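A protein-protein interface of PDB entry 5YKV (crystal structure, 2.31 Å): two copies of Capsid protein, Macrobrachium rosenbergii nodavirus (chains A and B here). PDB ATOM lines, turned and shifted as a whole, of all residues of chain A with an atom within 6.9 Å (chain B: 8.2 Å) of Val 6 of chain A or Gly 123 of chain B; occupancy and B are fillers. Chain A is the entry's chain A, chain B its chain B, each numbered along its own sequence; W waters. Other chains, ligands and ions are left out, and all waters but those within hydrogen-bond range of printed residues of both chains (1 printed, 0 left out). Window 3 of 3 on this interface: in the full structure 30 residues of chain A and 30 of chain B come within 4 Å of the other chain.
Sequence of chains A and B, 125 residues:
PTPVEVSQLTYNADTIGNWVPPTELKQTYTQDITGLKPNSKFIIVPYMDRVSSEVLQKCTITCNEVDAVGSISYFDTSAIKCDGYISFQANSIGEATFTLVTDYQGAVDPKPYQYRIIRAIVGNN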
ATOM      1  N   VAL A   4     -16.743  -5.718 -26.438  1.00  0.00           N
ATOM      2  CA  VAL A   4     -17.330  -5.767 -25.094  1.00  0.00           C
ATOM      3  C   VAL A   4     -18.513  -4.788 -25.100  1.00  0.00           C
ATOM      4  O   VAL A   4     -18.351  -3.640 -25.469  1.00  0.00           O
ATOM      5  CB  VAL A   4     -16.279  -5.453 -24.003  1.00  0.00           C
ATOM      6  CG1 VAL A   4     -16.893  -5.302 -22.626  1.00  0.00           C
ATOM      7  CG2 VAL A   4     -15.151  -6.474 -23.944  1.00  0.00           C
ATOM      8  N   GLU A   5     -19.714  -5.267 -24.746  1.00  0.00           N
ATOM      9  CA  GLU A   5     -20.880  -4.402 -24.727  1.00  0.00           C
ATOM     10  C   GLU A   5     -20.782  -3.543 -23.457  1.00  0.00           C
ATOM     11  O   GLU A   5     -20.258  -3.934 -22.436  1.00  0.00           O
ATOM     12  CB  GLU A   5     -22.206  -5.173 -24.865  1.00  0.00           C
ATOM     13  CG  GLU A   5     -23.410  -4.285 -25.306  1.00  0.00           C
ATOM     14  CD  GLU A   5     -23.321  -3.377 -26.553  1.00  0.00           C
ATOM     15  OE1 GLU A   5     -23.005  -3.897 -27.637  1.00  0.00           O
ATOM     16  OE2 GLU A   5     -23.607  -2.150 -26.463  1.00  0.00           O
ATOM     17  N   VAL A   6     -21.298  -2.337 -23.596  1.00  0.00           N
ATOM     18  CA  VAL A   6     -21.302  -1.245 -22.662  1.00  0.00           C
ATOM     19  C   VAL A   6     -21.698  -1.681 -21.239  1.00  0.00           C
ATOM     20  O   VAL A   6     -21.089  -1.273 -20.253  1.00  0.00           O
ATOM     21  CB  VAL A   6     -22.228  -0.192 -23.301  1.00  0.00           C
ATOM     22  CG1 VAL A   6     -23.145   0.501 -22.326  1.00  0.00           C
ATOM     23  CG2 VAL A   6     -21.419   0.793 -24.137  1.00  0.00           C
ATOM     24  N   SER A   7     -22.692  -2.549 -21.113  1.00  0.00           N
ATOM     25  CA  SER A   7     -23.120  -3.014 -19.799  1.00  0.00           C
ATOM     26  C   SER A   7     -22.028  -3.848 -19.121  1.00  0.00           C
ATOM     27  O   SER A   7     -22.163  -4.090 -17.966  1.00  0.00           O
ATOM     28  CB  SER A   7     -24.424  -3.786 -19.861  1.00  0.00           C
ATOM     29  OG  SER A   7     -25.476  -2.954 -20.329  1.00  0.00           O
ATOM     30  N   GLN A   8     -20.984  -4.299 -19.840  1.00  0.00           N
ATOM     31  CA  GLN A   8     -19.916  -5.131 -19.216  1.00  0.00           C
ATOM     32  C   GLN A   8     -18.615  -4.323 -19.021  1.00  0.00           C
ATOM     33  O   GLN A   8     -17.559  -4.930 -18.824  1.00  0.00           O
ATOM     34  CB  GLN A   8     -19.573  -6.388 -20.034  1.00  0.00           C
ATOM     35  CG  GLN A   8     -20.731  -7.022 -20.794  1.00  0.00           C
ATOM     36  CD  GLN A   8     -21.753  -7.579 -19.846  1.00  0.00           C
ATOM     37  OE1 GLN A   8     -21.402  -8.358 -18.961  1.00  0.00           O
ATOM     38  NE2 GLN A   8     -23.007  -7.163 -20.013  1.00  0.00           N
ATOM     39  N   LEU A   9     -18.698  -2.988 -19.062  1.00  0.00           N
ATOM     40  CA  LEU A   9     -17.578  -2.059 -18.838  1.00  0.00           C
ATOM     41  C   LEU A   9     -16.830  -2.472 -17.583  1.00  0.00           C
ATOM     42  O   LEU A   9     -17.450  -2.621 -16.550  1.00  0.00           O
ATOM     43  CB  LEU A   9     -18.089  -0.624 -18.669  1.00  0.00           C
ATOM     44  CG  LEU A   9     -17.064   0.413 -18.178  1.00  0.00           C
ATOM     45  CD1 LEU A   9     -15.951   0.618 -19.198  1.00  0.00           C
ATOM     46  CD2 LEU A   9     -17.737   1.760 -17.895  1.00  0.00           C
ATOM     47  N   THR A  10     -15.509  -2.652 -17.702  1.00  0.00           N
ATOM     48  CA  THR A  10     -14.633  -2.764 -16.541  1.00  0.00           C
ATOM     49  C   THR A  10     -13.414  -1.896 -16.809  1.00  0.00           C
ATOM     50  O   THR A  10     -13.228  -1.435 -17.903  1.00  0.00           O
ATOM     51  CB  THR A  10     -14.215  -4.208 -16.235  1.00  0.00           C
ATOM     52  OG1 THR A  10     -13.519  -4.730 -17.371  1.00  0.00           O
ATOM     53  CG2 THR A  10     -15.390  -5.109 -15.893  1.00  0.00           C
ATOM     54  N   ILE A 121     -12.242  -1.176 -20.574  1.00  0.00           N
ATOM     55  CA  ILE A 121     -12.428  -2.366 -21.381  1.00  0.00           C
ATOM     56  C   ILE A 121     -13.893  -2.426 -21.785  1.00  0.00           C
ATOM     57  O   ILE A 121     -14.750  -2.854 -21.037  1.00  0.00           O
ATOM     58  CB  ILE A 121     -11.964  -3.650 -20.681  1.00  0.00           C
ATOM     59  CG1 ILE A 121     -10.461  -3.601 -20.376  1.00  0.00           C
ATOM     60  CG2 ILE A 121     -12.324  -4.848 -21.549  1.00  0.00           C
ATOM     61  CD1 ILE A 121     -10.027  -4.605 -19.346  1.00  0.00           C
ATOM     62  N   VAL A 122     -14.123  -1.935 -22.994  1.00  0.00           N
ATOM     63  CA  VAL A 122     -15.375  -1.687 -23.537  1.00  0.00           C
ATOM     64  C   VAL A 122     -15.152  -1.518 -25.044  1.00  0.00           C
ATOM     65  O   VAL A 122     -14.050  -1.139 -25.507  1.00  0.00           O
ATOM     66  CB  VAL A 122     -16.020  -0.451 -22.888  1.00  0.00           C
ATOM     67  CG1 VAL A 122     -15.268   0.837 -23.200  1.00  0.00           C
ATOM     68  CG2 VAL A 122     -17.480  -0.329 -23.305  1.00  0.00           C
ATOM     69  N   GLY A 123     -16.171  -1.861 -25.829  1.00  0.00           N
ATOM     70  CA  GLY A 123     -16.007  -1.937 -27.280  1.00  0.00           C
ATOM     71  C   GLY A 123     -14.791  -2.761 -27.679  1.00  0.00           C
ATOM     72  O   GLY A 123     -14.543  -3.861 -27.148  1.00  0.00           O
ATOM     73  N   PRO B   1     -32.833   8.406 -22.807  1.00  0.00           N
ATOM     74  CA  PRO B   1     -31.365   8.471 -22.610  1.00  0.00           C
ATOM     75  C   PRO B   1     -30.580   7.785 -23.748  1.00  0.00           C
ATOM     76  O   PRO B   1     -30.616   6.557 -23.869  1.00  0.00           O
ATOM     77  CB  PRO B   1     -31.138   7.767 -21.259  1.00  0.00           C
ATOM     78  CG  PRO B   1     -32.407   6.937 -21.017  1.00  0.00           C
ATOM     79  CD  PRO B   1     -33.340   7.179 -22.192  1.00  0.00           C
ATOM     80  N   THR B   2     -29.899   8.577 -24.592  1.00  0.00           N
ATOM     81  CA  THR B   2     -29.106   8.026 -25.703  1.00  0.00           C
ATOM     82  C   THR B   2     -27.699   7.688 -25.227  1.00  0.00           C
ATOM     83  O   THR B   2     -26.930   8.568 -24.847  1.00  0.00           O
ATOM     84  CB  THR B   2     -28.943   8.971 -26.899  1.00  0.00           C
ATOM     85  OG1 THR B   2     -30.133   9.732 -27.077  1.00  0.00           O
ATOM     86  CG2 THR B   2     -28.625   8.203 -28.165  1.00  0.00           C
ATOM     87  N   PRO B   3     -27.312   6.401 -25.277  1.00  0.00           N
ATOM     88  CA  PRO B   3     -25.968   5.978 -24.879  1.00  0.00           C
ATOM     89  C   PRO B   3     -24.892   6.640 -25.751  1.00  0.00           C
ATOM     90  O   PRO B   3     -25.144   6.886 -26.915  1.00  0.00           O
ATOM     91  CB  PRO B   3     -25.988   4.459 -25.103  1.00  0.00           C
ATOM     92  CG  PRO B   3     -27.457   4.087 -25.072  1.00  0.00           C
ATOM     93  CD  PRO B   3     -28.166   5.277 -25.685  1.00  0.00           C
ATOM     94  N   VAL B   4     -23.747   6.985 -25.151  1.00  0.00           N
ATOM     95  CA  VAL B   4     -22.584   7.478 -25.868  1.00  0.00           C
ATOM     96  C   VAL B   4     -21.978   6.281 -26.606  1.00  0.00           C
ATOM     97  O   VAL B   4     -21.735   5.243 -25.991  1.00  0.00           O
ATOM     98  CB  VAL B   4     -21.555   8.108 -24.901  1.00  0.00           C
ATOM     99  CG1 VAL B   4     -20.210   8.369 -25.592  1.00  0.00           C
ATOM    100  CG2 VAL B   4     -22.081   9.388 -24.265  1.00  0.00           C
ATOM    101  N   GLU B   5     -21.701   6.434 -27.902  1.00  0.00           N
ATOM    102  CA  GLU B   5     -21.154   5.323 -28.700  1.00  0.00           C
ATOM    103  C   GLU B   5     -19.723   5.003 -28.253  1.00  0.00           C
ATOM    104  O   GLU B   5     -18.980   5.875 -27.829  1.00  0.00           O
ATOM    105  CB  GLU B   5     -21.191   5.657 -30.189  1.00  0.00           C
ATOM    106  CG  GLU B   5     -22.462   5.205 -30.874  1.00  0.00           C
ATOM    107  CD  GLU B   5     -22.573   5.701 -32.307  1.00  0.00           C
ATOM    108  OE1 GLU B   5     -23.678   6.131 -32.713  1.00  0.00           O
ATOM    109  OE2 GLU B   5     -21.543   5.658 -33.017  1.00  0.00           O
ATOM    110  N   VAL B   6     -19.341   3.735 -28.393  1.00  0.00           N
ATOM    111  CA  VAL B   6     -18.040   3.270 -27.987  1.00  0.00           C
ATOM    112  C   VAL B   6     -16.930   4.050 -28.720  1.00  0.00           C
ATOM    113  O   VAL B   6     -15.927   4.396 -28.114  1.00  0.00           O
ATOM    114  CB  VAL B   6     -17.905   1.752 -28.186  1.00  0.00           C
ATOM    115  CG1 VAL B   6     -16.463   1.329 -27.977  1.00  0.00           C
ATOM    116  CG2 VAL B   6     -18.823   0.971 -27.260  1.00  0.00           C
ATOM    117  N   SER B   7     -17.108   4.363 -30.007  1.00  0.00           N
ATOM    118  CA  SER B   7     -16.103   5.136 -30.760  1.00  0.00           C
ATOM    119  C   SER B   7     -15.863   6.517 -30.125  1.00  0.00           C
ATOM    120  O   SER B   7     -14.881   7.194 -30.455  1.00  0.00           O
ATOM    121  CB  SER B   7     -16.513   5.293 -32.212  1.00  0.00           C
ATOM    122  OG  SER B   7     -17.306   6.460 -32.392  1.00  0.00           O
ATOM    123  N   GLN B   8     -16.790   6.976 -29.269  1.00  0.00           N
ATOM    124  CA  GLN B   8     -16.697   8.317 -28.645  1.00  0.00           C
ATOM    125  C   GLN B   8     -16.178   8.235 -27.196  1.00  0.00           C
ATOM    126  O   GLN B   8     -16.204   9.228 -26.483  1.00  0.00           O
ATOM    127  CB  GLN B   8     -18.065   9.017 -28.700  1.00  0.00           C
ATOM    128  CG  GLN B   8     -18.614   9.247 -30.109  1.00  0.00           C
ATOM    129  CD  GLN B   8     -17.587   9.971 -30.938  1.00  0.00           C
ATOM    130  OE1 GLN B   8     -17.299  11.124 -30.658  1.00  0.00           O
ATOM    131  NE2 GLN B   8     -16.982   9.276 -31.902  1.00  0.00           N
ATOM    132  N   LEU B   9     -15.692   7.072 -26.751  1.00  0.00           N
ATOM    133  CA  LEU B   9     -15.124   6.912 -25.388  1.00  0.00           C
ATOM    134  C   LEU B   9     -14.131   8.052 -25.064  1.00  0.00           C
ATOM    135  O   LEU B   9     -13.336   8.441 -25.911  1.00  0.00           O
ATOM    136  CB  LEU B   9     -14.459   5.537 -25.326  1.00  0.00           C
ATOM    137  CG  LEU B   9     -13.628   5.269 -24.081  1.00  0.00           C
ATOM    138  CD1 LEU B   9     -14.527   5.161 -22.857  1.00  0.00           C
ATOM    139  CD2 LEU B   9     -12.804   4.017 -24.268  1.00  0.00           C
ATOM    140  N   LYS B  37     -22.836   9.843 -10.546  1.00  0.00           N
ATOM    141  CA  LYS B  37     -23.909   9.413 -11.420  1.00  0.00           C
ATOM    142  C   LYS B  37     -24.352   8.036 -10.945  1.00  0.00           C
ATOM    143  O   LYS B  37     -23.538   7.124 -10.821  1.00  0.00           O
ATOM    144  CB  LYS B  37     -23.455   9.387 -12.874  1.00  0.00           C
ATOM    145  CG  LYS B  37     -24.551   9.140 -13.899  1.00  0.00           C
ATOM    146  CD  LYS B  37     -23.986   9.137 -15.300  1.00  0.00           C
ATOM    147  CE  LYS B  37     -25.005   9.408 -16.392  1.00  0.00           C
ATOM    148  NZ  LYS B  37     -25.863   8.226 -16.612  1.00  0.00           N
ATOM    149  N   SER B  40     -23.150   4.328 -12.136  1.00  0.00           N
ATOM    150  CA  SER B  40     -21.912   4.419 -12.968  1.00  0.00           C
ATOM    151  C   SER B  40     -20.745   3.671 -12.323  1.00  0.00           C
ATOM    152  O   SER B  40     -20.696   3.494 -11.128  1.00  0.00           O
ATOM    153  CB  SER B  40     -21.500   5.813 -13.243  1.00  0.00           C
ATOM    154  OG  SER B  40     -22.362   6.386 -14.194  1.00  0.00           O
ATOM    155  N   LYS B  41     -19.800   3.247 -13.166  1.00  0.00           N
ATOM    156  CA  LYS B  41     -18.662   2.530 -12.736  1.00  0.00           C
ATOM    157  C   LYS B  41     -17.415   3.421 -12.801  1.00  0.00           C
ATOM    158  O   LYS B  41     -17.102   4.039 -13.800  1.00  0.00           O
ATOM    159  CB  LYS B  41     -18.531   1.300 -13.621  1.00  0.00           C
ATOM    160  CG  LYS B  41     -19.686   0.319 -13.533  1.00  0.00           C
ATOM    161  CD  LYS B  41     -19.485  -0.898 -14.400  1.00  0.00           C
ATOM    162  CE  LYS B  41     -20.663  -1.853 -14.380  1.00  0.00           C
ATOM    163  NZ  LYS B  41     -20.772  -2.579 -15.672  1.00  0.00           N
ATOM    164  N   ARG B 119     -13.896   8.294 -14.518  1.00  0.00           N
ATOM    165  CA  ARG B 119     -15.161   7.815 -15.113  1.00  0.00           C
ATOM    166  C   ARG B 119     -14.989   7.717 -16.642  1.00  0.00           C
ATOM    167  O   ARG B 119     -14.700   8.701 -17.306  1.00  0.00           O
ATOM    168  CB  ARG B 119     -16.252   8.835 -14.765  1.00  0.00           C
ATOM    169  CG  ARG B 119     -17.641   8.578 -15.332  1.00  0.00           C
ATOM    170  CD  ARG B 119     -18.560   9.794 -15.157  1.00  0.00           C
ATOM    171  NE  ARG B 119     -19.795   9.628 -15.915  1.00  0.00           N
ATOM    172  CZ  ARG B 119     -20.451  10.597 -16.549  1.00  0.00           C
ATOM    173  NH1 ARG B 119     -21.464  10.299 -17.352  1.00  0.00           N
ATOM    174  NH2 ARG B 119     -20.095  11.858 -16.379  1.00  0.00           N
ATOM    175  N   ALA B 120     -15.129   6.518 -17.199  1.00  0.00           N
ATOM    176  CA  ALA B 120     -15.254   6.358 -18.632  1.00  0.00           C
ATOM    177  C   ALA B 120     -16.637   6.877 -19.045  1.00  0.00           C
ATOM    178  O   ALA B 120     -17.632   6.500 -18.454  1.00  0.00           O
ATOM    179  CB  ALA B 120     -15.064   4.910 -18.981  1.00  0.00           C
ATOM    180  N   ILE B 121     -16.669   7.848 -19.964  1.00  0.00           N
ATOM    181  CA  ILE B 121     -17.884   8.379 -20.528  1.00  0.00           C
ATOM    182  C   ILE B 121     -18.153   7.593 -21.809  1.00  0.00           C
ATOM    183  O   ILE B 121     -17.551   7.851 -22.861  1.00  0.00           O
ATOM    184  CB  ILE B 121     -17.751   9.891 -20.740  1.00  0.00           C
ATOM    185  CG1 ILE B 121     -17.393  10.554 -19.406  1.00  0.00           C
ATOM    186  CG2 ILE B 121     -19.026  10.468 -21.355  1.00  0.00           C
ATOM    187  CD1 ILE B 121     -17.494  12.059 -19.398  1.00  0.00           C
ATOM    188  N   VAL B 122     -18.977   6.557 -21.641  1.00  0.00           N
ATOM    189  CA  VAL B 122     -19.334   5.616 -22.663  1.00  0.00           C
ATOM    190  C   VAL B 122     -20.654   4.941 -22.259  1.00  0.00           C
ATOM    191  O   VAL B 122     -20.968   4.775 -21.059  1.00  0.00           O
ATOM    192  CB  VAL B 122     -18.203   4.586 -22.854  1.00  0.00           C
ATOM    193  CG1 VAL B 122     -18.149   3.598 -21.704  1.00  0.00           C
ATOM    194  CG2 VAL B 122     -18.330   3.836 -24.179  1.00  0.00           C
ATOM    195  N   GLY B 123     -21.450   4.534 -23.250  1.00  0.00           N
ATOM    196  CA  GLY B 123     -22.754   3.992 -22.930  1.00  0.00           C
ATOM    197  C   GLY B 123     -23.537   4.976 -22.073  1.00  0.00           C
ATOM    198  O   GLY B 123     -23.613   6.124 -22.396  1.00  0.00           O
ATOM    199  N   ASN B 124     -24.104   4.501 -20.963  1.00  0.00           N
ATOM    200  CA  ASN B 124     -24.802   5.346 -20.024  1.00  0.00           C
ATOM    201  C   ASN B 124     -23.937   5.513 -18.762  1.00  0.00           C
ATOM    202  O   ASN B 124     -24.430   5.921 -17.724  1.00  0.00           O
ATOM    203  CB  ASN B 124     -26.184   4.753 -19.698  1.00  0.00           C
ATOM    204  CG  ASN B 124     -27.247   4.983 -20.766  1.00  0.00           C
ATOM    205  OD1 ASN B 124     -27.215   5.959 -21.513  1.00  0.00           O
ATOM    206  ND2 ASN B 124     -28.212   4.088 -20.851  1.00  0.00           N
ATOM    207  N   ASN B 125     -22.663   5.100 -18.824  1.00  0.00           N
ATOM    208  CA  ASN B 125     -21.724   5.364 -17.760  1.00  0.00           C
ATOM    209  C   ASN B 125     -21.442   6.872 -17.749  1.00  0.00           C
ATOM    210  O   ASN B 125     -21.252   7.416 -16.652  1.00  0.00           O
ATOM    211  CB  ASN B 125     -20.431   4.565 -17.901  1.00  0.00           C
ATOM    212  CG  ASN B 125     -19.773   4.266 -16.573  1.00  0.00           C
ATOM    213  OD1 ASN B 125     -20.333   3.513 -15.769  1.00  0.00           O
ATOM    214  ND2 ASN B 125     -18.584   4.817 -16.336  1.00  0.00           N
HETATM  215  O   HOH W   1     -21.930  -0.628 -17.833  1.00  0.00           O
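Printed residues of chain A that touch a printed residue of chain B: Val 6, Ser 7, Leu 9 and Gly 123. Of the 19 printed residues of chain B, 4 touch a printed residue of chain A. Hydrophobic or aromatic side chains of chain B within 4 Å of the printed part of chain A: Val 6.
Water W1 lies within hydrogen-bond range of the backbone carbonyl oxygen (O) of Val 6 of chain A, the side-chain amino group (NZ) of Lys 41 of chain B and the backbone carbonyl oxygen (O) of Ser 7 of chain A.
Among the printed residues, merely in contact across the chains: Val 6 of chain A with Gly 123 of chain B (3.6 Å), Leu 9 of chain A with Asn 125 of chain B (3.5 Å) and Gly 123 of chain A with Val 6 of chain B (3.4 Å).
The backbone carbonyl oxygen (O) of Val 4 of chain B is in hydrogen-bond range of the backbone NH (N) of Gly 123 of chain B (2.8 Å). The backbone carbonyl oxygen (O) of Ala 120 of chain B lies within hydrogen-bond range of the side-chain amide nitrogen (ND2) of Asn 125 of chain B, 2.9 Å away. O of Asn 125 of chain B lies within hydrogen-bond range of NE of Arg 119 of chain B (2.7 Å). The side-chain hydroxyl (OG) of Ser 40 of chain B is in hydrogen-bond range of the backbone carbonyl oxygen (O) of Asn 125 of chain B (2.9 Å). The backbone carbonyl oxygen (O) of Val 4 of chain A lies within hydrogen-bond range of the backbone NH (N) of Gly 123 of chain A (2.8 Å). N of Lys 41 of chain B lies within hydrogen-bond range of OD1 of Asn 125 of chain B (2.7 Å).
NZ of Lys 41 of chain B lies within hydrogen-bond range of O of Ser 7 of chain A (3.1 Å). The side-chain amino group (NZ) of Lys 41 of chain B sits close to the backbone carbonyl oxygen (O) of Leu 9 of chain A (3.4 Å).
Val 6 of chain A touches Gly 123 of chain B, and with the chains exchanged Gly 123 of chain A touches Val 6 of chain B. Of the 5 pairs that touch across the chains among the printed residues, 2 have their exchanged pair printed and touching as well.
Of chain B, only Lys 41 (3.1 Å) comes within 4 Å of Ser 7 of chain A. Val 122 of chain A touches none of the printed residues of chain B. Printed residues of chain A within 4 Å of Val 6 of chain B: Gly 123 (3.4 Å). Of the printed residues of chain A, Lys 41 of chain B touches Ser 7 and Leu 9. Of the printed residues of chain A, Asn 125 of chain B touches Leu 9. The nearest residue of chain B that does not touch Val 6 of chain A is Val 6 of chain B (4.1 Å). The nearest printed residue of chain A that does not touch Val 6 of chain B is Val 6 of chain A (4.1 Å).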
